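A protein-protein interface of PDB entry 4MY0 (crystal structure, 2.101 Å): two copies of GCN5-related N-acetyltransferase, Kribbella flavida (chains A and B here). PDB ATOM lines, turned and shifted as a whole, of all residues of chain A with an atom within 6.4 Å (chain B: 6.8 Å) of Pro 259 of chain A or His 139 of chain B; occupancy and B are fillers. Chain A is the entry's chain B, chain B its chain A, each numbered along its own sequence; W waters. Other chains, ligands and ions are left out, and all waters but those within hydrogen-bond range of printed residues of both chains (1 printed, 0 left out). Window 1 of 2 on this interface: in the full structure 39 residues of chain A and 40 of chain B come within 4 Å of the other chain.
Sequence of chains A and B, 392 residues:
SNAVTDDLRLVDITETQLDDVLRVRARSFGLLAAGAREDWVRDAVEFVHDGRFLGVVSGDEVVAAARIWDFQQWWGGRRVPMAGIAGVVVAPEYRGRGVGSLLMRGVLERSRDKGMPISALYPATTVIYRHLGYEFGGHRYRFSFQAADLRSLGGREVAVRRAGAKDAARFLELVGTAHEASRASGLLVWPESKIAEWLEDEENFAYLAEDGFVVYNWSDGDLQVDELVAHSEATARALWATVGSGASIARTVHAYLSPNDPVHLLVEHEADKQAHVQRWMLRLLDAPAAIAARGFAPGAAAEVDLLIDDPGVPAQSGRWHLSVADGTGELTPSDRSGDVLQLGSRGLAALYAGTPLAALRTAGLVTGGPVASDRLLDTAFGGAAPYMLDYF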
ATOM      1  N   TYR A 141      20.283  17.732  12.436  1.00  0.00           N
ATOM      2  CA  TYR A 141      20.762  18.792  11.559  1.00  0.00           C
ATOM      3  C   TYR A 141      20.368  20.147  12.130  1.00  0.00           C
ATOM      4  O   TYR A 141      19.217  20.322  12.530  1.00  0.00           O
ATOM      5  CB  TYR A 141      20.083  18.659  10.202  1.00  0.00           C
ATOM      6  CG  TYR A 141      20.508  17.465   9.355  1.00  0.00           C
ATOM      7  CD1 TYR A 141      21.612  17.542   8.514  1.00  0.00           C
ATOM      8  CD2 TYR A 141      19.780  16.280   9.373  1.00  0.00           C
ATOM      9  CE1 TYR A 141      21.991  16.457   7.716  1.00  0.00           C
ATOM     10  CE2 TYR A 141      20.151  15.189   8.577  1.00  0.00           C
ATOM     11  CZ  TYR A 141      21.258  15.287   7.761  1.00  0.00           C
ATOM     12  OH  TYR A 141      21.636  14.218   6.971  1.00  0.00           O
ATOM     13  N   PHE A 143      20.351  24.111  10.704  1.00  0.00           N
ATOM     14  CA  PHE A 143      20.623  25.039   9.600  1.00  0.00           C
ATOM     15  C   PHE A 143      20.355  26.481  10.015  1.00  0.00           C
ATOM     16  O   PHE A 143      19.535  26.734  10.899  1.00  0.00           O
ATOM     17  CB  PHE A 143      19.768  24.700   8.375  1.00  0.00           C
ATOM     18  CG  PHE A 143      20.119  23.380   7.736  1.00  0.00           C
ATOM     19  CD1 PHE A 143      21.216  23.279   6.880  1.00  0.00           C
ATOM     20  CD2 PHE A 143      19.356  22.244   7.984  1.00  0.00           C
ATOM     21  CE1 PHE A 143      21.554  22.066   6.281  1.00  0.00           C
ATOM     22  CE2 PHE A 143      19.683  21.011   7.376  1.00  0.00           C
ATOM     23  CZ  PHE A 143      20.778  20.928   6.534  1.00  0.00           C
ATOM     24  N   LEU A 257      15.957  20.762  11.938  1.00  0.00           N
ATOM     25  CA  LEU A 257      15.022  20.127  11.010  1.00  0.00           C
ATOM     26  C   LEU A 257      15.759  19.238  10.009  1.00  0.00           C
ATOM     27  O   LEU A 257      16.985  19.209   9.995  1.00  0.00           O
ATOM     28  CB  LEU A 257      14.163  21.167  10.298  1.00  0.00           C
ATOM     29  CG  LEU A 257      14.698  22.561   9.987  1.00  0.00           C
ATOM     30  CD1 LEU A 257      15.623  22.541   8.798  1.00  0.00           C
ATOM     31  CD2 LEU A 257      13.504  23.423   9.704  1.00  0.00           C
ATOM     32  N   SER A 258      15.004  18.527   9.174  1.00  0.00           N
ATOM     33  CA  SER A 258      15.595  17.683   8.134  1.00  0.00           C
ATOM     34  C   SER A 258      16.094  18.481   6.935  1.00  0.00           C
ATOM     35  O   SER A 258      15.599  19.573   6.661  1.00  0.00           O
ATOM     36  CB  SER A 258      14.587  16.643   7.648  1.00  0.00           C
ATOM     37  OG  SER A 258      15.013  16.067   6.424  1.00  0.00           O
ATOM     38  N   PRO A 259      17.074  17.926   6.195  1.00  0.00           N
ATOM     39  CA  PRO A 259      17.459  18.581   4.934  1.00  0.00           C
ATOM     40  C   PRO A 259      16.345  18.459   3.898  1.00  0.00           C
ATOM     41  O   PRO A 259      16.385  19.169   2.879  1.00  0.00           O
ATOM     42  CB  PRO A 259      18.703  17.806   4.480  1.00  0.00           C
ATOM     43  CG  PRO A 259      18.647  16.496   5.212  1.00  0.00           C
ATOM     44  CD  PRO A 259      17.925  16.761   6.507  1.00  0.00           C
ATOM     45  N   ASN A 260      15.358  17.593   4.156  1.00  0.00           N
ATOM     46  CA  ASN A 260      14.147  17.551   3.310  1.00  0.00           C
ATOM     47  C   ASN A 260      13.001  18.478   3.741  1.00  0.00           C
ATOM     48  O   ASN A 260      11.911  18.405   3.183  1.00  0.00           O
ATOM     49  CB  ASN A 260      13.600  16.128   3.197  1.00  0.00           C
ATOM     50  CG  ASN A 260      14.495  15.225   2.382  1.00  0.00           C
ATOM     51  OD1 ASN A 260      15.169  15.672   1.448  1.00  0.00           O
ATOM     52  ND2 ASN A 260      14.514  13.942   2.735  1.00  0.00           N
ATOM     53  N   ASP A 261      13.238  19.340   4.724  1.00  0.00           N
ATOM     54  CA  ASP A 261      12.170  20.234   5.195  1.00  0.00           C
ATOM     55  C   ASP A 261      11.720  21.202   4.086  1.00  0.00           C
ATOM     56  O   ASP A 261      12.545  21.691   3.304  1.00  0.00           O
ATOM     57  CB  ASP A 261      12.607  21.011   6.438  1.00  0.00           C
ATOM     58  CG  ASP A 261      11.421  21.655   7.169  1.00  0.00           C
ATOM     59  OD1 ASP A 261      10.949  21.051   8.145  1.00  0.00           O
ATOM     60  OD2 ASP A 261      10.944  22.738   6.748  1.00  0.00           O
ATOM     61  N   HIS A 264      13.388  24.920   2.992  1.00  0.00           N
ATOM     62  CA  HIS A 264      14.416  25.084   1.966  1.00  0.00           C
ATOM     63  C   HIS A 264      13.805  25.422   0.614  1.00  0.00           C
ATOM     64  O   HIS A 264      14.426  26.099  -0.203  1.00  0.00           O
ATOM     65  CB  HIS A 264      15.272  23.814   1.847  1.00  0.00           C
ATOM     66  CG  HIS A 264      15.920  23.399   3.136  1.00  0.00           C
ATOM     67  ND1 HIS A 264      16.986  24.083   3.692  1.00  0.00           N
ATOM     68  CD2 HIS A 264      15.659  22.365   3.973  1.00  0.00           C
ATOM     69  CE1 HIS A 264      17.347  23.485   4.817  1.00  0.00           C
ATOM     70  NE2 HIS A 264      16.563  22.438   5.007  1.00  0.00           N
ATOM     71  N   ALA A 385      15.116   9.756   5.288  1.00  0.00           N
ATOM     72  CA  ALA A 385      16.314   9.591   6.109  1.00  0.00           C
ATOM     73  C   ALA A 385      15.964   9.870   7.563  1.00  0.00           C
ATOM     74  O   ALA A 385      15.279  10.849   7.853  1.00  0.00           O
ATOM     75  CB  ALA A 385      17.400  10.531   5.633  1.00  0.00           C
ATOM     76  N   TYR A 387      16.093  11.197  11.242  1.00  0.00           N
ATOM     77  CA  TYR A 387      16.706  12.333  11.923  1.00  0.00           C
ATOM     78  C   TYR A 387      15.976  12.558  13.226  1.00  0.00           C
ATOM     79  O   TYR A 387      14.895  12.005  13.449  1.00  0.00           O
ATOM     80  CB  TYR A 387      16.646  13.612  11.070  1.00  0.00           C
ATOM     81  CG  TYR A 387      15.225  14.149  10.902  1.00  0.00           C
ATOM     82  CD1 TYR A 387      14.775  15.251  11.638  1.00  0.00           C
ATOM     83  CD2 TYR A 387      14.339  13.548  10.004  1.00  0.00           C
ATOM     84  CE1 TYR A 387      13.463  15.742  11.477  1.00  0.00           C
ATOM     85  CE2 TYR A 387      13.032  14.020   9.839  1.00  0.00           C
ATOM     86  CZ  TYR A 387      12.603  15.115  10.579  1.00  0.00           C
ATOM     87  OH  TYR A 387      11.311  15.567  10.411  1.00  0.00           O
ATOM     88  N   TYR B 122      24.514  25.374  -9.605  1.00  0.00           N
ATOM     89  CA  TYR B 122      24.615  25.877  -8.236  1.00  0.00           C
ATOM     90  C   TYR B 122      24.311  27.365  -8.288  1.00  0.00           C
ATOM     91  O   TYR B 122      25.077  28.142  -8.868  1.00  0.00           O
ATOM     92  CB  TYR B 122      26.038  25.709  -7.698  1.00  0.00           C
ATOM     93  CG  TYR B 122      26.428  24.314  -7.246  1.00  0.00           C
ATOM     94  CD1 TYR B 122      26.298  23.932  -5.909  1.00  0.00           C
ATOM     95  CD2 TYR B 122      26.970  23.405  -8.133  1.00  0.00           C
ATOM     96  CE1 TYR B 122      26.681  22.668  -5.485  1.00  0.00           C
ATOM     97  CE2 TYR B 122      27.352  22.138  -7.726  1.00  0.00           C
ATOM     98  CZ  TYR B 122      27.205  21.779  -6.397  1.00  0.00           C
ATOM     99  OH  TYR B 122      27.595  20.531  -5.981  1.00  0.00           O
ATOM    100  N   PHE B 136      15.804  23.134  -6.005  1.00  0.00           N
ATOM    101  CA  PHE B 136      16.837  22.355  -5.308  1.00  0.00           C
ATOM    102  C   PHE B 136      16.568  20.862  -5.448  1.00  0.00           C
ATOM    103  O   PHE B 136      15.445  20.407  -5.236  1.00  0.00           O
ATOM    104  CB  PHE B 136      16.927  22.734  -3.826  1.00  0.00           C
ATOM    105  CG  PHE B 136      17.571  24.079  -3.579  1.00  0.00           C
ATOM    106  CD1 PHE B 136      18.781  24.408  -4.175  1.00  0.00           C
ATOM    107  CD2 PHE B 136      16.956  25.016  -2.756  1.00  0.00           C
ATOM    108  CE1 PHE B 136      19.385  25.669  -3.946  1.00  0.00           C
ATOM    109  CE2 PHE B 136      17.542  26.255  -2.513  1.00  0.00           C
ATOM    110  CZ  PHE B 136      18.754  26.586  -3.117  1.00  0.00           C
ATOM    111  N   GLY B 137      17.604  20.114  -5.817  1.00  0.00           N
ATOM    112  CA  GLY B 137      17.465  18.708  -6.134  1.00  0.00           C
ATOM    113  C   GLY B 137      18.406  17.827  -5.327  1.00  0.00           C
ATOM    114  O   GLY B 137      18.205  16.615  -5.241  1.00  0.00           O
ATOM    115  N   GLY B 138      19.446  18.417  -4.748  1.00  0.00           N
ATOM    116  CA  GLY B 138      20.400  17.625  -3.985  1.00  0.00           C
ATOM    117  C   GLY B 138      21.474  18.438  -3.297  1.00  0.00           C
ATOM    118  O   GLY B 138      21.458  19.670  -3.337  1.00  0.00           O
ATOM    119  N   HIS B 139      22.424  17.741  -2.676  1.00  0.00           N
ATOM    120  CA  HIS B 139      23.368  18.393  -1.788  1.00  0.00           C
ATOM    121  C   HIS B 139      24.815  18.110  -2.163  1.00  0.00           C
ATOM    122  O   HIS B 139      25.102  17.162  -2.902  1.00  0.00           O
ATOM    123  CB  HIS B 139      23.117  17.955  -0.334  1.00  0.00           C
ATOM    124  CG  HIS B 139      21.757  18.324   0.184  1.00  0.00           C
ATOM    125  ND1 HIS B 139      20.652  17.513   0.024  1.00  0.00           N
ATOM    126  CD2 HIS B 139      21.321  19.428   0.840  1.00  0.00           C
ATOM    127  CE1 HIS B 139      19.598  18.097   0.566  1.00  0.00           C
ATOM    128  NE2 HIS B 139      19.976  19.260   1.070  1.00  0.00           N
ATOM    129  N   ARG B 140      25.713  18.956  -1.658  1.00  0.00           N
ATOM    130  CA  ARG B 140      27.146  18.652  -1.631  1.00  0.00           C
ATOM    131  C   ARG B 140      27.636  18.843  -0.189  1.00  0.00           C
ATOM    132  O   ARG B 140      27.526  19.939   0.380  1.00  0.00           O
ATOM    133  CB  ARG B 140      27.898  19.582  -2.583  1.00  0.00           C
ATOM    134  CG  ARG B 140      29.406  19.314  -2.675  1.00  0.00           C
ATOM    135  CD  ARG B 140      30.035  20.415  -3.509  1.00  0.00           C
ATOM    136  NE  ARG B 140      31.441  20.182  -3.822  1.00  0.00           N
ATOM    137  CZ  ARG B 140      32.394  21.089  -3.614  1.00  0.00           C
ATOM    138  NH1 ARG B 140      33.647  20.819  -3.929  1.00  0.00           N
ATOM    139  NH2 ARG B 140      32.090  22.265  -3.070  1.00  0.00           N
ATOM    140  N   TYR B 141      28.163  17.771   0.389  1.00  0.00           N
ATOM    141  CA  TYR B 141      28.563  17.730   1.794  1.00  0.00           C
ATOM    142  C   TYR B 141      30.073  17.690   1.922  1.00  0.00           C
ATOM    143  O   TYR B 141      30.731  16.892   1.251  1.00  0.00           O
ATOM    144  CB  TYR B 141      28.053  16.442   2.441  1.00  0.00           C
ATOM    145  CG  TYR B 141      26.558  16.267   2.489  1.00  0.00           C
ATOM    146  CD1 TYR B 141      25.822  16.710   3.581  1.00  0.00           C
ATOM    147  CD2 TYR B 141      25.884  15.611   1.458  1.00  0.00           C
ATOM    148  CE1 TYR B 141      24.435  16.523   3.638  1.00  0.00           C
ATOM    149  CE2 TYR B 141      24.515  15.425   1.509  1.00  0.00           C
ATOM    150  CZ  TYR B 141      23.799  15.877   2.594  1.00  0.00           C
ATOM    151  OH  TYR B 141      22.434  15.685   2.633  1.00  0.00           O
ATOM    152  N   PRO B 259      26.509  11.623   3.333  1.00  0.00           N
ATOM    153  CA  PRO B 259      26.376  11.342   4.767  1.00  0.00           C
ATOM    154  C   PRO B 259      26.163   9.837   5.019  1.00  0.00           C
ATOM    155  O   PRO B 259      26.317   9.375   6.160  1.00  0.00           O
ATOM    156  CB  PRO B 259      25.150  12.172   5.188  1.00  0.00           C
ATOM    157  CG  PRO B 259      24.388  12.422   3.921  1.00  0.00           C
ATOM    158  CD  PRO B 259      25.384  12.415   2.799  1.00  0.00           C
ATOM    159  N   VAL B 277      27.295  22.267   3.953  1.00  0.00           N
ATOM    160  CA  VAL B 277      26.194  21.654   3.227  1.00  0.00           C
ATOM    161  C   VAL B 277      25.773  22.656   2.152  1.00  0.00           C
ATOM    162  O   VAL B 277      25.257  23.731   2.474  1.00  0.00           O
ATOM    163  CB  VAL B 277      25.007  21.327   4.176  1.00  0.00           C
ATOM    164  CG1 VAL B 277      23.852  20.689   3.407  1.00  0.00           C
ATOM    165  CG2 VAL B 277      25.460  20.422   5.337  1.00  0.00           C
ATOM    166  N   GLN B 278      26.034  22.323   0.888  1.00  0.00           N
ATOM    167  CA  GLN B 278      25.601  23.154  -0.241  1.00  0.00           C
ATOM    168  C   GLN B 278      24.468  22.452  -0.992  1.00  0.00           C
ATOM    169  O   GLN B 278      24.322  21.228  -0.897  1.00  0.00           O
ATOM    170  CB  GLN B 278      26.755  23.385  -1.226  1.00  0.00           C
ATOM    171  CG  GLN B 278      27.799  24.396  -0.790  1.00  0.00           C
ATOM    172  CD  GLN B 278      29.094  24.279  -1.596  1.00  0.00           C
ATOM    173  OE1 GLN B 278      29.740  23.226  -1.616  1.00  0.00           O
ATOM    174  NE2 GLN B 278      29.473  25.358  -2.260  1.00  0.00           N
ATOM    175  N   ARG B 279      23.688  23.230  -1.742  1.00  0.00           N
ATOM    176  CA  ARG B 279      22.575  22.709  -2.530  1.00  0.00           C
ATOM    177  C   ARG B 279      22.737  23.074  -3.988  1.00  0.00           C
ATOM    178  O   ARG B 279      23.169  24.181  -4.312  1.00  0.00           O
ATOM    179  CB  ARG B 279      21.265  23.318  -2.036  1.00  0.00           C
ATOM    180  CG  ARG B 279      20.898  22.876  -0.635  1.00  0.00           C
ATOM    181  CD  ARG B 279      19.775  23.751  -0.021  1.00  0.00           C
ATOM    182  NE  ARG B 279      19.662  23.360   1.375  1.00  0.00           N
ATOM    183  CZ  ARG B 279      20.527  23.743   2.309  1.00  0.00           C
ATOM    184  NH1 ARG B 279      21.531  24.563   1.996  1.00  0.00           N
ATOM    185  NH2 ARG B 279      20.391  23.315   3.555  1.00  0.00           N
ATOM    186  N   TRP B 280      22.376  22.146  -4.867  1.00  0.00           N
ATOM    187  CA  TRP B 280      22.336  22.442  -6.285  1.00  0.00           C
ATOM    188  C   TRP B 280      20.911  22.239  -6.800  1.00  0.00           C
ATOM    189  O   TRP B 280      20.130  21.472  -6.219  1.00  0.00           O
ATOM    190  CB  TRP B 280      23.341  21.583  -7.062  1.00  0.00           C
ATOM    191  CG  TRP B 280      23.376  20.148  -6.648  1.00  0.00           C
ATOM    192  CD1 TRP B 280      24.222  19.586  -5.728  1.00  0.00           C
ATOM    193  CD2 TRP B 280      22.564  19.075  -7.153  1.00  0.00           C
ATOM    194  NE1 TRP B 280      23.979  18.236  -5.624  1.00  0.00           N
ATOM    195  CE2 TRP B 280      22.962  17.896  -6.482  1.00  0.00           C
ATOM    196  CE3 TRP B 280      21.530  19.000  -8.099  1.00  0.00           C
ATOM    197  CZ2 TRP B 280      22.366  16.642  -6.733  1.00  0.00           C
ATOM    198  CZ3 TRP B 280      20.935  17.759  -8.345  1.00  0.00           C
ATOM    199  CH2 TRP B 280      21.356  16.597  -7.663  1.00  0.00           C
ATOM    200  N   ALA B 385      19.824   9.408  -1.179  1.00  0.00           N
ATOM    201  CA  ALA B 385      19.639  10.844  -1.319  1.00  0.00           C
ATOM    202  C   ALA B 385      20.637  11.349  -2.344  1.00  0.00           C
ATOM    203  O   ALA B 385      21.796  10.939  -2.335  1.00  0.00           O
ATOM    204  CB  ALA B 385      19.835  11.549   0.023  1.00  0.00           C
ATOM    205  N   PRO B 386      20.181  12.223  -3.250  1.00  0.00           N
ATOM    206  CA  PRO B 386      21.094  12.640  -4.315  1.00  0.00           C
ATOM    207  C   PRO B 386      22.154  13.625  -3.821  1.00  0.00           C
ATOM    208  O   PRO B 386      21.876  14.536  -3.033  1.00  0.00           O
ATOM    209  CB  PRO B 386      20.160  13.246  -5.380  1.00  0.00           C
ATOM    210  CG  PRO B 386      18.874  13.575  -4.643  1.00  0.00           C
ATOM    211  CD  PRO B 386      18.787  12.671  -3.458  1.00  0.00           C
ATOM    212  N   TYR B 387      23.387  13.411  -4.266  1.00  0.00           N
ATOM    213  CA  TYR B 387      24.483  14.272  -3.855  1.00  0.00           C
ATOM    214  C   TYR B 387      25.490  14.384  -4.972  1.00  0.00           C
ATOM    215  O   TYR B 387      25.462  13.608  -5.937  1.00  0.00           O
ATOM    216  CB  TYR B 387      25.169  13.747  -2.587  1.00  0.00           C
ATOM    217  CG  TYR B 387      26.011  12.499  -2.799  1.00  0.00           C
ATOM    218  CD1 TYR B 387      27.398  12.587  -2.927  1.00  0.00           C
ATOM    219  CD2 TYR B 387      25.419  11.240  -2.860  1.00  0.00           C
ATOM    220  CE1 TYR B 387      28.175  11.444  -3.109  1.00  0.00           C
ATOM    221  CE2 TYR B 387      26.174  10.098  -3.046  1.00  0.00           C
ATOM    222  CZ  TYR B 387      27.556  10.207  -3.172  1.00  0.00           C
ATOM    223  OH  TYR B 387      28.323   9.081  -3.350  1.00  0.00           O
ATOM    224  N   MET B 388      26.390  15.345  -4.823  1.00  0.00           N
ATOM    225  CA  MET B 388      27.432  15.574  -5.805  1.00  0.00           C
ATOM    226  C   MET B 388      28.746  15.756  -5.047  1.00  0.00           C
ATOM    227  O   MET B 388      28.733  16.181  -3.884  1.00  0.00           O
ATOM    228  CB  MET B 388      27.105  16.856  -6.556  1.00  0.00           C
ATOM    229  CG  MET B 388      27.723  16.968  -7.901  1.00  0.00           C
ATOM    230  SD  MET B 388      26.950  18.530  -8.764  1.00  0.00           S
ATOM    231  CE  MET B 388      25.172  17.825  -9.041  1.00  0.00           C
ATOM    232  N   LEU B 389      29.871  15.454  -5.696  1.00  0.00           N
ATOM    233  CA  LEU B 389      31.179  15.707  -5.091  1.00  0.00           C
ATOM    234  C   LEU B 389      31.748  17.058  -5.549  1.00  0.00           C
ATOM    235  O   LEU B 389      32.554  17.675  -4.851  1.00  0.00           O
ATOM    236  CB  LEU B 389      32.154  14.584  -5.463  1.00  0.00           C
ATOM    237  CG  LEU B 389      31.767  13.179  -5.011  1.00  0.00           C
ATOM    238  CD1 LEU B 389      32.831  12.200  -5.441  1.00  0.00           C
ATOM    239  CD2 LEU B 389      31.585  13.137  -3.511  1.00  0.00           C
HETATM  240  O   HOH W   1      18.621  21.295   2.555  1.00  0.00           O
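Positions printed for both chains: 141, 259, 385 and 387.
Of the 5 pairs that touch across the chains among the printed residues, none has its exchanged pair printed and touching as well.
A ring nitrogen (ND1) of His 264 of chain A sits close to the guanidinium group of Arg 279 of chain B (3.5 Å).
Water W1 lies within hydrogen-bond range of the guanidinium group (NE) of Arg 279 of chain B, a ring nitrogen (NE2) of His 139 of chain B, the backbone carbonyl oxygen (O) of Pro 259 of chain A and a ring nitrogen (NE2) of His 264 of chain A.
CG1 of Val 277 of chain B touches CE1 of Phe 143 of chain A, at 3.9 Å.
Phe 143 of chain A touches Arg 279 of chain B.
Pro 259 of chain A touches His 139 of chain B.
His 264 of chain A touches Phe 136 of chain B.
Of the printed residues of chain B, Phe 143 of chain A touches Val 277 and Arg 279.
Of chain B, only His 139 comes within 4 Å of Pro 259 of chain A.
Of the printed residues of chain B, His 264 of chain A touches Phe 136 and Arg 279.
His 139 of chain B touches one residue of chain A.
Of the printed residues of chain A, Val 277 of chain B touches Phe 143.
Printed residues of chain A within 4 Å of Arg 279 of chain B: Phe 143 (3.2 Å) and His 264 (3.3 Å).
The nearest residue of chain B that does not touch Pro 259 of chain A is Tyr 141 of chain B (4.7 Å).
The nearest printed residue of chain A that does not touch Phe 136 of chain B is Pro 259 of chain A (7.6 Å).
Of the 10 printed residues of chain A, 3 touch a printed residue of chain B.
Hydrophobic or aromatic side chains of chain A within 4 Å of the printed part of chain B: Phe 143, Pro 259 and His 264.
Along chain A the printed residues that touch a printed residue of chain B span positions 143 to 264.
Hydrophobic or aromatic side chains of chain B within 4 Å of the printed part of chain A: Phe 136, His 139 and Val 277.
Among the printed residues, 5 pairs touch across the chains.
Among the printed residues, no Asp or Glu carboxylate lies within 4 Å of a Lys or Arg side-chain nitrogen of the other chain.
The indole nitrogen of Trp 280 of chain B lies within hydrogen-bond range of the backbone carbonyl oxygen of His 139 of chain B (3.1 Å).
O of Pro 386 of chain B lies within hydrogen-bond range of N of His 139 of chain B (3.3 Å).
The backbone carbonyl oxygen (O) of His 139 of chain B lies within hydrogen-bond range of the backbone NH (N) of Met 388 of chain B, 2.9 Å away.
The backbone carbonyl oxygen (O) of Ser 258 of chain A is in hydrogen-bond range of a ring nitrogen (NE2) of His 264 of chain A.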
